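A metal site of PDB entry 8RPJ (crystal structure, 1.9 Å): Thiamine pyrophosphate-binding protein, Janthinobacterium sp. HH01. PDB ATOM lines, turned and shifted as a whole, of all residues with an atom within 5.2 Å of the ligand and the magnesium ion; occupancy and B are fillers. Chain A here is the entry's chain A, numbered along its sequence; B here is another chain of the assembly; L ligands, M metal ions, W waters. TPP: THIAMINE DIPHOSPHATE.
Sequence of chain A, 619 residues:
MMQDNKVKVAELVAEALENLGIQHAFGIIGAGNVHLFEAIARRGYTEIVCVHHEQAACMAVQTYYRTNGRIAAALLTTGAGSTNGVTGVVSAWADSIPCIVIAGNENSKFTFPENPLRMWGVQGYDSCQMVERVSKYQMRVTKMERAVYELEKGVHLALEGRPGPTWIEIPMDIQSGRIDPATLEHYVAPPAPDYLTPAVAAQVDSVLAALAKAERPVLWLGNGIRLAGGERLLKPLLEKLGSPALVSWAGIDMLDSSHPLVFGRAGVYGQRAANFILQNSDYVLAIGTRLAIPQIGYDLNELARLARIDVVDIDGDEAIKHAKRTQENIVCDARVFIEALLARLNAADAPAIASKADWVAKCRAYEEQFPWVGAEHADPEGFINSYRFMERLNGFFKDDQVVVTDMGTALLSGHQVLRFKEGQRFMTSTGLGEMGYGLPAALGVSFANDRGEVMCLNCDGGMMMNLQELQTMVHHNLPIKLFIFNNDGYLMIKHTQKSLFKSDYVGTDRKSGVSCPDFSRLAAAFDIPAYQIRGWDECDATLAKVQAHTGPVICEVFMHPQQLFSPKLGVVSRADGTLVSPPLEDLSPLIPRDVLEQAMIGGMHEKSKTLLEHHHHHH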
ATOM      1  N   ASP A 406      -8.919   3.410  32.765  1.00  0.00           N
ATOM      2  CA  ASP A 406      -7.983   3.780  31.707  1.00  0.00           C
ATOM      3  C   ASP A 406      -6.788   2.835  31.811  1.00  0.00           C
ATOM      4  O   ASP A 406      -6.910   1.720  32.331  1.00  0.00           O
ATOM      5  CB  ASP A 406      -7.580   5.253  31.830  1.00  0.00           C
ATOM      6  CG  ASP A 406      -7.374   5.914  30.468  1.00  0.00           C
ATOM      7  OD1 ASP A 406      -8.336   6.437  29.880  1.00  0.00           O
ATOM      8  OD2 ASP A 406      -6.219   5.891  29.972  1.00  0.00           O
ATOM      9  N   MET A 407      -5.635   3.255  31.305  1.00  0.00           N
ATOM     10  CA  MET A 407      -4.432   2.435  31.341  1.00  0.00           C
ATOM     11  C   MET A 407      -3.637   2.771  32.599  1.00  0.00           C
ATOM     12  O   MET A 407      -4.224   3.177  33.611  1.00  0.00           O
ATOM     13  CB  MET A 407      -3.636   2.643  30.059  1.00  0.00           C
ATOM     14  CG  MET A 407      -4.444   2.345  28.796  1.00  0.00           C
ATOM     15  SD  MET A 407      -4.967   0.604  28.710  1.00  0.00           S
ATOM     16  CE  MET A 407      -6.751   0.765  28.807  1.00  0.00           C
ATOM     17  N   GLY A 408      -2.320   2.598  32.560  1.00  0.00           N
ATOM     18  CA  GLY A 408      -1.452   3.060  33.614  1.00  0.00           C
ATOM     19  C   GLY A 408      -1.781   2.498  34.992  1.00  0.00           C
ATOM     20  O   GLY A 408      -2.196   1.345  35.150  1.00  0.00           O
ATOM     21  N   THR A 409      -1.578   3.343  36.008  1.00  0.00           N
ATOM     22  CA  THR A 409      -1.808   2.920  37.385  1.00  0.00           C
ATOM     23  C   THR A 409      -3.203   2.333  37.565  1.00  0.00           C
ATOM     24  O   THR A 409      -3.367   1.303  38.233  1.00  0.00           O
ATOM     25  CB  THR A 409      -1.633   4.100  38.339  1.00  0.00           C
ATOM     26  OG1 THR A 409      -0.285   4.581  38.274  1.00  0.00           O
ATOM     27  CG2 THR A 409      -1.975   3.707  39.768  1.00  0.00           C
ATOM     28  N   ALA A 410      -4.209   2.989  36.993  1.00  0.00           N
ATOM     29  CA  ALA A 410      -5.579   2.502  37.145  1.00  0.00           C
ATOM     30  C   ALA A 410      -5.706   1.082  36.626  1.00  0.00           C
ATOM     31  O   ALA A 410      -6.297   0.223  37.284  1.00  0.00           O
ATOM     32  CB  ALA A 410      -6.545   3.439  36.406  1.00  0.00           C
ATOM     33  N   GLY A 433      -5.320  -1.477  24.366  1.00  0.00           N
ATOM     34  CA  GLY A 433      -4.655  -0.810  25.461  1.00  0.00           C
ATOM     35  C   GLY A 433      -4.475   0.677  25.266  1.00  0.00           C
ATOM     36  O   GLY A 433      -3.447   1.223  25.655  1.00  0.00           O
ATOM     37  N   GLU A 434      -5.462   1.346  24.673  1.00  0.00           N
ATOM     38  CA  GLU A 434      -5.317   2.758  24.357  1.00  0.00           C
ATOM     39  C   GLU A 434      -5.562   3.619  25.590  1.00  0.00           C
ATOM     40  O   GLU A 434      -6.526   3.412  26.333  1.00  0.00           O
ATOM     41  CB  GLU A 434      -6.281   3.170  23.232  1.00  0.00           C
ATOM     42  CG  GLU A 434      -7.755   3.245  23.621  1.00  0.00           C
ATOM     43  CD  GLU A 434      -8.496   1.946  23.386  1.00  0.00           C
ATOM     44  OE1 GLU A 434      -7.935   0.867  23.670  1.00  0.00           O
ATOM     45  OE2 GLU A 434      -9.659   2.002  22.928  1.00  0.00           O
ATOM     46  N   MET A 435      -4.684   4.600  25.800  1.00  0.00           N
ATOM     47  CA  MET A 435      -4.969   5.680  26.724  1.00  0.00           C
ATOM     48  C   MET A 435      -6.217   6.423  26.267  1.00  0.00           C
ATOM     49  O   MET A 435      -6.479   6.568  25.069  1.00  0.00           O
ATOM     50  CB  MET A 435      -3.801   6.640  26.804  1.00  0.00           C
ATOM     51  CG  MET A 435      -2.558   6.043  27.387  1.00  0.00           C
ATOM     52  SD  MET A 435      -1.171   7.164  27.166  1.00  0.00           S
ATOM     53  CE  MET A 435      -1.626   8.486  28.276  1.00  0.00           C
ATOM     54  N   CYS A 459      -6.182   8.413  34.980  1.00  0.00           N
ATOM     55  CA  CYS A 459      -4.786   8.765  35.136  1.00  0.00           C
ATOM     56  C   CYS A 459      -4.547  10.152  34.592  1.00  0.00           C
ATOM     57  O   CYS A 459      -5.269  10.635  33.721  1.00  0.00           O
ATOM     58  CB  CYS A 459      -3.881   7.779  34.395  1.00  0.00           C
ATOM     59  SG  CYS A 459      -4.121   6.105  34.945  1.00  0.00           S
ATOM     60  N   ASP A 460      -3.497  10.796  35.087  1.00  0.00           N
ATOM     61  CA  ASP A 460      -3.229  12.165  34.665  1.00  0.00           C
ATOM     62  C   ASP A 460      -2.903  12.217  33.179  1.00  0.00           C
ATOM     63  O   ASP A 460      -3.339  13.128  32.479  1.00  0.00           O
ATOM     64  CB  ASP A 460      -2.151  12.802  35.547  1.00  0.00           C
ATOM     65  CG  ASP A 460      -0.860  11.992  35.658  1.00  0.00           C
ATOM     66  OD1 ASP A 460      -0.749  10.859  35.144  1.00  0.00           O
ATOM     67  OD2 ASP A 460       0.077  12.542  36.287  1.00  0.00           O
ATOM     68  N   GLY A 461      -2.199  11.218  32.654  1.00  0.00           N
ATOM     69  CA  GLY A 461      -1.941  11.159  31.234  1.00  0.00           C
ATOM     70  C   GLY A 461      -3.134  10.750  30.390  1.00  0.00           C
ATOM     71  O   GLY A 461      -3.494  11.433  29.429  1.00  0.00           O
ATOM     72  N   GLY A 462      -3.756   9.635  30.779  1.00  0.00           N
ATOM     73  CA  GLY A 462      -4.896   9.129  30.031  1.00  0.00           C
ATOM     74  C   GLY A 462      -6.082  10.084  30.023  1.00  0.00           C
ATOM     75  O   GLY A 462      -6.853  10.107  29.058  1.00  0.00           O
ATOM     76  N   MET A 465      -6.401  12.395  26.714  1.00  0.00           N
ATOM     77  CA  MET A 465      -6.722  11.977  25.343  1.00  0.00           C
ATOM     78  C   MET A 465      -8.187  12.253  24.999  1.00  0.00           C
ATOM     79  O   MET A 465      -8.500  12.608  23.863  1.00  0.00           O
ATOM     80  CB  MET A 465      -6.412  10.498  25.129  1.00  0.00           C
ATOM     81  CG  MET A 465      -5.016  10.247  24.590  1.00  0.00           C
ATOM     82  SD  MET A 465      -3.853  10.443  25.943  1.00  0.00           S
ATOM     83  CE  MET A 465      -2.308  10.191  25.101  1.00  0.00           C
ATOM     84  N   PHE A 485      -5.323   9.303  39.077  1.00  0.00           N
ATOM     85  CA  PHE A 485      -4.028   9.069  39.718  1.00  0.00           C
ATOM     86  C   PHE A 485      -2.994  10.048  39.172  1.00  0.00           C
ATOM     87  O   PHE A 485      -2.595   9.957  38.004  1.00  0.00           O
ATOM     88  CB  PHE A 485      -3.577   7.623  39.502  1.00  0.00           C
ATOM     89  CG  PHE A 485      -4.372   6.641  40.305  1.00  0.00           C
ATOM     90  CD1 PHE A 485      -4.102   6.442  41.644  1.00  0.00           C
ATOM     91  CD2 PHE A 485      -5.419   5.948  39.720  1.00  0.00           C
ATOM     92  CE1 PHE A 485      -4.836   5.554  42.392  1.00  0.00           C
ATOM     93  CE2 PHE A 485      -6.164   5.056  40.473  1.00  0.00           C
ATOM     94  CZ  PHE A 485      -5.870   4.863  41.801  1.00  0.00           C
ATOM     95  N   ASN A 487       0.726  11.333  39.069  1.00  0.00           N
ATOM     96  CA  ASN A 487       2.086  10.870  39.321  1.00  0.00           C
ATOM     97  C   ASN A 487       3.108  11.569  38.412  1.00  0.00           C
ATOM     98  O   ASN A 487       4.105  10.947  38.029  1.00  0.00           O
ATOM     99  CB  ASN A 487       2.192   9.341  39.175  1.00  0.00           C
ATOM    100  CG  ASN A 487       1.538   8.826  37.895  1.00  0.00           C
ATOM    101  OD1 ASN A 487       1.446   9.534  36.885  1.00  0.00           O
ATOM    102  ND2 ASN A 487       1.106   7.569  37.920  1.00  0.00           N
ATOM    103  N   GLY A 489       3.062  12.614  35.229  1.00  0.00           N
ATOM    104  CA  GLY A 489       3.225  12.166  33.867  1.00  0.00           C
ATOM    105  C   GLY A 489       3.015  10.695  33.642  1.00  0.00           C
ATOM    106  O   GLY A 489       2.074  10.098  34.176  1.00  0.00           O
ATOM    107  N   TYR A 490       3.915  10.078  32.858  1.00  0.00           N
ATOM    108  CA  TYR A 490       3.714   8.746  32.317  1.00  0.00           C
ATOM    109  C   TYR A 490       4.513   7.710  33.107  1.00  0.00           C
ATOM    110  O   TYR A 490       5.583   7.280  32.697  1.00  0.00           O
ATOM    111  CB  TYR A 490       4.155   8.718  30.859  1.00  0.00           C
ATOM    112  CG  TYR A 490       3.376   9.582  29.908  1.00  0.00           C
ATOM    113  CD1 TYR A 490       2.126  10.084  30.249  1.00  0.00           C
ATOM    114  CD2 TYR A 490       3.885   9.871  28.659  1.00  0.00           C
ATOM    115  CE1 TYR A 490       1.412  10.872  29.361  1.00  0.00           C
ATOM    116  CE2 TYR A 490       3.180  10.649  27.767  1.00  0.00           C
ATOM    117  CZ  TYR A 490       1.949  11.147  28.113  1.00  0.00           C
ATOM    118  OH  TYR A 490       1.257  11.920  27.210  1.00  0.00           O
ATOM    119  N   LEU A 491       3.955   7.274  34.236  1.00  0.00           N
ATOM    120  CA  LEU A 491       4.720   6.423  35.128  1.00  0.00           C
ATOM    121  C   LEU A 491       5.098   5.108  34.462  1.00  0.00           C
ATOM    122  O   LEU A 491       6.233   4.637  34.604  1.00  0.00           O
ATOM    123  CB  LEU A 491       3.940   6.181  36.408  1.00  0.00           C
ATOM    124  CG  LEU A 491       4.631   5.323  37.466  1.00  0.00           C
ATOM    125  CD1 LEU A 491       6.019   5.782  37.771  1.00  0.00           C
ATOM    126  CD2 LEU A 491       3.760   5.357  38.723  1.00  0.00           C
ATOM    127  N   MET A 492       4.174   4.490  33.734  1.00  0.00           N
ATOM    128  CA  MET A 492       4.506   3.217  33.114  1.00  0.00           C
ATOM    129  C   MET A 492       5.721   3.351  32.195  1.00  0.00           C
ATOM    130  O   MET A 492       6.593   2.478  32.178  1.00  0.00           O
ATOM    131  CB  MET A 492       3.321   2.666  32.346  1.00  0.00           C
ATOM    132  CG  MET A 492       3.441   1.187  32.137  1.00  0.00           C
ATOM    133  SD  MET A 492       1.969   0.438  31.450  1.00  0.00           S
ATOM    134  CE  MET A 492       2.616  -1.167  31.009  1.00  0.00           C
ATOM    135  N   ILE A 493       5.793   4.451  31.439  1.00  0.00           N
ATOM    136  CA  ILE A 493       6.916   4.599  30.520  1.00  0.00           C
ATOM    137  C   ILE A 493       8.186   5.025  31.278  1.00  0.00           C
ATOM    138  O   ILE A 493       9.291   4.667  30.864  1.00  0.00           O
ATOM    139  CB  ILE A 493       6.569   5.586  29.395  1.00  0.00           C
ATOM    140  CG1 ILE A 493       5.242   5.191  28.721  1.00  0.00           C
ATOM    141  CG2 ILE A 493       7.691   5.637  28.367  1.00  0.00           C
ATOM    142  CD1 ILE A 493       5.210   3.785  28.122  1.00  0.00           C
ATOM    143  N   PHE A 565       5.439  -0.418  39.896  1.00  0.00           N
ATOM    144  CA  PHE A 565       4.354  -1.347  39.631  1.00  0.00           C
ATOM    145  C   PHE A 565       4.915  -2.742  39.855  1.00  0.00           C
ATOM    146  O   PHE A 565       5.935  -3.116  39.265  1.00  0.00           O
ATOM    147  CB  PHE A 565       3.847  -1.202  38.198  1.00  0.00           C
ATOM    148  CG  PHE A 565       3.205   0.117  37.910  1.00  0.00           C
ATOM    149  CD1 PHE A 565       2.292   0.683  38.793  1.00  0.00           C
ATOM    150  CD2 PHE A 565       3.503   0.789  36.735  1.00  0.00           C
ATOM    151  CE1 PHE A 565       1.697   1.900  38.496  1.00  0.00           C
ATOM    152  CE2 PHE A 565       2.914   1.999  36.449  1.00  0.00           C
ATOM    153  CZ  PHE A 565       2.011   2.555  37.329  1.00  0.00           C
ATOM    154  N   ILE B  28       3.942  11.252  20.800  1.00  0.00           N
ATOM    155  CA  ILE B  28       3.732  10.712  22.137  1.00  0.00           C
ATOM    156  C   ILE B  28       4.540   9.429  22.248  1.00  0.00           C
ATOM    157  O   ILE B  28       4.545   8.600  21.331  1.00  0.00           O
ATOM    158  CB  ILE B  28       2.244  10.468  22.434  1.00  0.00           C
ATOM    159  CG1 ILE B  28       1.449  11.767  22.239  1.00  0.00           C
ATOM    160  CG2 ILE B  28       2.043   9.921  23.856  1.00  0.00           C
ATOM    161  CD1 ILE B  28      -0.022  11.695  22.636  1.00  0.00           C
ATOM    162  N   ILE B  29       5.201   9.267  23.383  1.00  0.00           N
ATOM    163  CA  ILE B  29       6.067   8.130  23.618  1.00  0.00           C
ATOM    164  C   ILE B  29       5.246   6.887  23.917  1.00  0.00           C
ATOM    165  O   ILE B  29       4.065   6.942  24.289  1.00  0.00           O
ATOM    166  CB  ILE B  29       7.042   8.447  24.768  1.00  0.00           C
ATOM    167  CG1 ILE B  29       8.243   7.508  24.767  1.00  0.00           C
ATOM    168  CG2 ILE B  29       6.303   8.384  26.099  1.00  0.00           C
ATOM    169  CD1 ILE B  29       9.374   8.019  25.639  1.00  0.00           C
ATOM    170  N   GLY B  30       5.880   5.738  23.729  1.00  0.00           N
ATOM    171  CA  GLY B  30       5.361   4.434  24.112  1.00  0.00           C
ATOM    172  C   GLY B  30       6.476   3.437  23.908  1.00  0.00           C
ATOM    173  O   GLY B  30       7.540   3.774  23.368  1.00  0.00           O
ATOM    174  N   GLU B  54      -2.221  12.094  19.606  1.00  0.00           N
ATOM    175  CA  GLU B  54      -1.383  11.962  18.411  1.00  0.00           C
ATOM    176  C   GLU B  54      -1.959  12.683  17.211  1.00  0.00           C
ATOM    177  O   GLU B  54      -1.211  13.083  16.301  1.00  0.00           O
ATOM    178  CB  GLU B  54      -1.181  10.467  18.112  1.00  0.00           C
ATOM    179  CG  GLU B  54      -0.261   9.741  19.100  1.00  0.00           C
ATOM    180  CD  GLU B  54      -0.961   9.166  20.325  1.00  0.00           C
ATOM    181  OE1 GLU B  54      -2.159   9.446  20.547  1.00  0.00           O
ATOM    182  OE2 GLU B  54      -0.286   8.431  21.073  1.00  0.00           O
ATOM    183  N   THR B  77       3.574   5.801  18.360  1.00  0.00           N
ATOM    184  CA  THR B  77       3.863   4.481  18.890  1.00  0.00           C
ATOM    185  C   THR B  77       2.865   3.449  18.370  1.00  0.00           C
ATOM    186  O   THR B  77       1.955   3.747  17.575  1.00  0.00           O
ATOM    187  CB  THR B  77       3.915   4.507  20.425  1.00  0.00           C
ATOM    188  OG1 THR B  77       4.545   3.302  20.890  1.00  0.00           O
ATOM    189  CG2 THR B  77       2.534   4.617  21.055  1.00  0.00           C
ATOM    190  N   ALA B  80      -2.776   2.288  19.347  1.00  0.00           N
ATOM    191  CA  ALA B  80      -3.553   3.524  19.328  1.00  0.00           C
ATOM    192  C   ALA B  80      -2.690   4.752  19.108  1.00  0.00           C
ATOM    193  O   ALA B  80      -3.215   5.786  18.686  1.00  0.00           O
ATOM    194  CB  ALA B  80      -4.336   3.653  20.639  1.00  0.00           C
ATOM    195  N   GLY B  81      -1.391   4.677  19.382  1.00  0.00           N
ATOM    196  CA  GLY B  81      -0.510   5.759  18.980  1.00  0.00           C
ATOM    197  C   GLY B  81      -0.553   6.031  17.496  1.00  0.00           C
ATOM    198  O   GLY B  81      -0.435   7.187  17.062  1.00  0.00           O
ATOM    199  N   ASN B  84      -4.492   6.921  16.272  1.00  0.00           N
ATOM    200  CA  ASN B  84      -4.856   8.279  16.662  1.00  0.00           C
ATOM    201  C   ASN B  84      -4.325   9.327  15.706  1.00  0.00           C
ATOM    202  O   ASN B  84      -4.823  10.458  15.711  1.00  0.00           O
ATOM    203  CB  ASN B  84      -4.336   8.576  18.067  1.00  0.00           C
ATOM    204  CG  ASN B  84      -5.306   8.185  19.161  1.00  0.00           C
ATOM    205  OD1 ASN B  84      -6.392   7.656  18.897  1.00  0.00           O
ATOM    206  ND2 ASN B  84      -4.914   8.420  20.407  1.00  0.00           N
ATOM    207  N   GLN B 123      -0.270  -5.530  20.844  1.00  0.00           N
ATOM    208  CA  GLN B 123      -1.306  -4.571  20.487  1.00  0.00           C
ATOM    209  C   GLN B 123      -1.047  -3.846  19.172  1.00  0.00           C
ATOM    210  O   GLN B 123      -1.487  -2.707  18.993  1.00  0.00           O
ATOM    211  CB  GLN B 123      -1.478  -3.521  21.604  1.00  0.00           C
ATOM    212  CG  GLN B 123      -0.189  -2.848  22.043  1.00  0.00           C
ATOM    213  CD  GLN B 123      -0.356  -2.067  23.327  1.00  0.00           C
ATOM    214  OE1 GLN B 123      -0.990  -2.530  24.276  1.00  0.00           O
ATOM    215  NE2 GLN B 123       0.188  -0.853  23.365  1.00  0.00           N
HETATM  216  N1' TPP L   1      -0.741   6.735  23.020  1.00  0.00           N
HETATM  217  C2' TPP L   1      -1.904   6.066  23.171  1.00  0.00           C
HETATM  218  CM2 TPP L   1      -3.109   6.636  22.499  1.00  0.00           C
HETATM  219  N3' TPP L   1      -2.060   4.945  23.871  1.00  0.00           N
HETATM  220  C4' TPP L   1      -0.980   4.423  24.491  1.00  0.00           C
HETATM  221  N4' TPP L   1      -1.166   3.289  25.173  1.00  0.00           N
HETATM  222  C5' TPP L   1       0.289   5.064  24.398  1.00  0.00           C
HETATM  223  C6' TPP L   1       0.317   6.211  23.642  1.00  0.00           C
HETATM  224  C7' TPP L   1       1.544   4.533  25.062  1.00  0.00           C
HETATM  225  N3  TPP L   1       1.462   4.507  26.555  1.00  0.00           N
HETATM  226  C2  TPP L   1       1.207   3.415  27.250  1.00  0.00           C
HETATM  227  S1  TPP L   1       1.185   3.712  28.902  1.00  0.00           S
HETATM  228  C5  TPP L   1       1.567   5.371  28.653  1.00  0.00           C
HETATM  229  C4  TPP L   1       1.682   5.641  27.336  1.00  0.00           C
HETATM  230  CM4 TPP L   1       1.991   6.958  26.713  1.00  0.00           C
HETATM  231  C6  TPP L   1       1.678   6.314  29.819  1.00  0.00           C
HETATM  232  C7  TPP L   1       0.433   6.311  30.660  1.00  0.00           C
HETATM  233  O7  TPP L   1       0.454   7.443  31.566  1.00  0.00           O
HETATM  234  PA  TPP L   1      -0.709   7.765  32.565  1.00  0.00           P
HETATM  235  O1A TPP L   1      -0.440   9.047  33.259  1.00  0.00           O
HETATM  236  O2A TPP L   1      -2.020   7.598  31.829  1.00  0.00           O
HETATM  237  O3A TPP L   1      -0.521   6.572  33.554  1.00  0.00           O
HETATM  238  PB  TPP L   1       0.526   6.060  34.610  1.00  0.00           P
HETATM  239  O1B TPP L   1       1.395   4.991  34.040  1.00  0.00           O
HETATM  240  O2B TPP L   1      -0.298   5.668  35.830  1.00  0.00           O
HETATM  241  O3B TPP L   1       1.292   7.335  34.938  1.00  0.00           O
HETATM  242 MG    MG M   1       0.475   9.222  35.050  1.00  0.00          MG
HETATM  243  O   HOH W   1       0.700   1.124  25.144  1.00  0.00           O
HETATM  244  O   HOH W   2      -3.736   5.808  31.455  1.00  0.00           O
HETATM  245  O   HOH W   3      -1.218   8.316  36.069  1.00  0.00           O
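The backbone NH (N) of Leu 491 lies within hydrogen-bond range of an oxygen (O1B) of the ligand (3.4 Å).
An oxygen (O1B) of the ligand lies within hydrogen-bond range of the backbone NH (N) of Met 492 (2.8 Å).
N of Gly 461 lies close to O1A of the ligand (2.9 Å).
The backbone carbonyl oxygen (O) of Gly 433 is in hydrogen-bond range of a nitrogen (N4') of the ligand (3.1 Å).
N3' of the ligand sits at hydrogen-bond distance from N of Met 435.
An oxygen (O2B) of the ligand lies within hydrogen-bond range of the side-chain hydroxyl (OG1) of Thr 409, 2.7 Å away.
An oxygen (O2A) of the ligand is in hydrogen-bond range of the backbone NH of Gly 462 (2.9 Å).
An oxygen (O2B) of the ligand sits at hydrogen-bond distance from the backbone NH of Thr 409, at 2.7 Å.
N1' of the ligand lies within hydrogen-bond range of OE2 of Glu 54 of chain B (2.6 Å).
SG of Cys 459 lies within hydrogen-bond range of O of Met 407, 3.2 Å away.
The side-chain amide nitrogen (ND2) of Asn 84 of chain B sits at hydrogen-bond distance from the side-chain carboxylate (OE1) of Glu 54 of chain B (2.9 Å).
The backbone NH (N) of Asp 460 is in hydrogen-bond range of the backbone carbonyl oxygen (O) of Phe 485, at 3.2 Å.
SG of Cys 459 is in hydrogen-bond range of N of Ala 410, at 3.7 Å.
The side-chain amide nitrogen of Asn 487 is in hydrogen-bond range of the side-chain hydroxyl of Thr 409, at 3.3 Å.
Merely in contact with the ligand: Cys 459 (3.2 Å), Ile 29 of chain B (3.2 Å), Asn 84 of chain B (3.3 Å), Tyr 490 (3.4 Å), Gly 408 (3.5 Å), Ile 493 (3.7 Å), Ala 80 of chain B (3.7 Å), Thr 77 of chain B (3.8 Å), Gly 30 of chain B (3.9 Å) and Glu 434 (3.95 Å).
Hydrophobic or aromatic side chains within 4 Å of the ligand: Met 435, Tyr 490, Leu 491, Met 492, Ile 493 and Ala 80 of chain B.
Within 4 Å of the ligand: Gly 408, Thr 409, Gly 433, Glu 434, Met 435, Cys 459, Asp 460, Gly 461, Gly 462, Asn 487, Gly 489, Tyr 490, Leu 491, Met 492, Ile 493, Ile 29 of chain B, Gly 30 of chain B, Glu 54 of chain B, Thr 77 of chain B, Ala 80 of chain B and Asn 84 of chain B.
The nearest printed residue that does not touch the ligand is Gly 81 of chain B (4.1 Å).
Three residues have an atom within 4 Å of the magnesium ion: Asp 460, Asn 487 and Gly 489.
The magnesium ion is bound by O1A of the ligand, O of Gly 489, OD1 of Asp 460, O3B of the ligand, OD1 of Asn 487 and water W3.
The magnesium ion has six donor atoms within binding distance.
Water W3 lies within hydrogen-bond range of O2B of the ligand (2.8 Å), O of Phe 485 (2.9 Å) and ND2 of Asn 487 (3.1 Å).
Water W2 lies within hydrogen-bond range of O2A of the ligand (2.5 Å), OD2 of Asp 406 (2.9 Å), N of Met 407 (3.2 Å) and SG of Cys 459 (3.5 Å).
Water W1 lies within hydrogen-bond range of the side-chain amide nitrogen of Gln 123 of chain B (2.7 Å) and a nitrogen (N4') of the ligand (2.9 Å).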
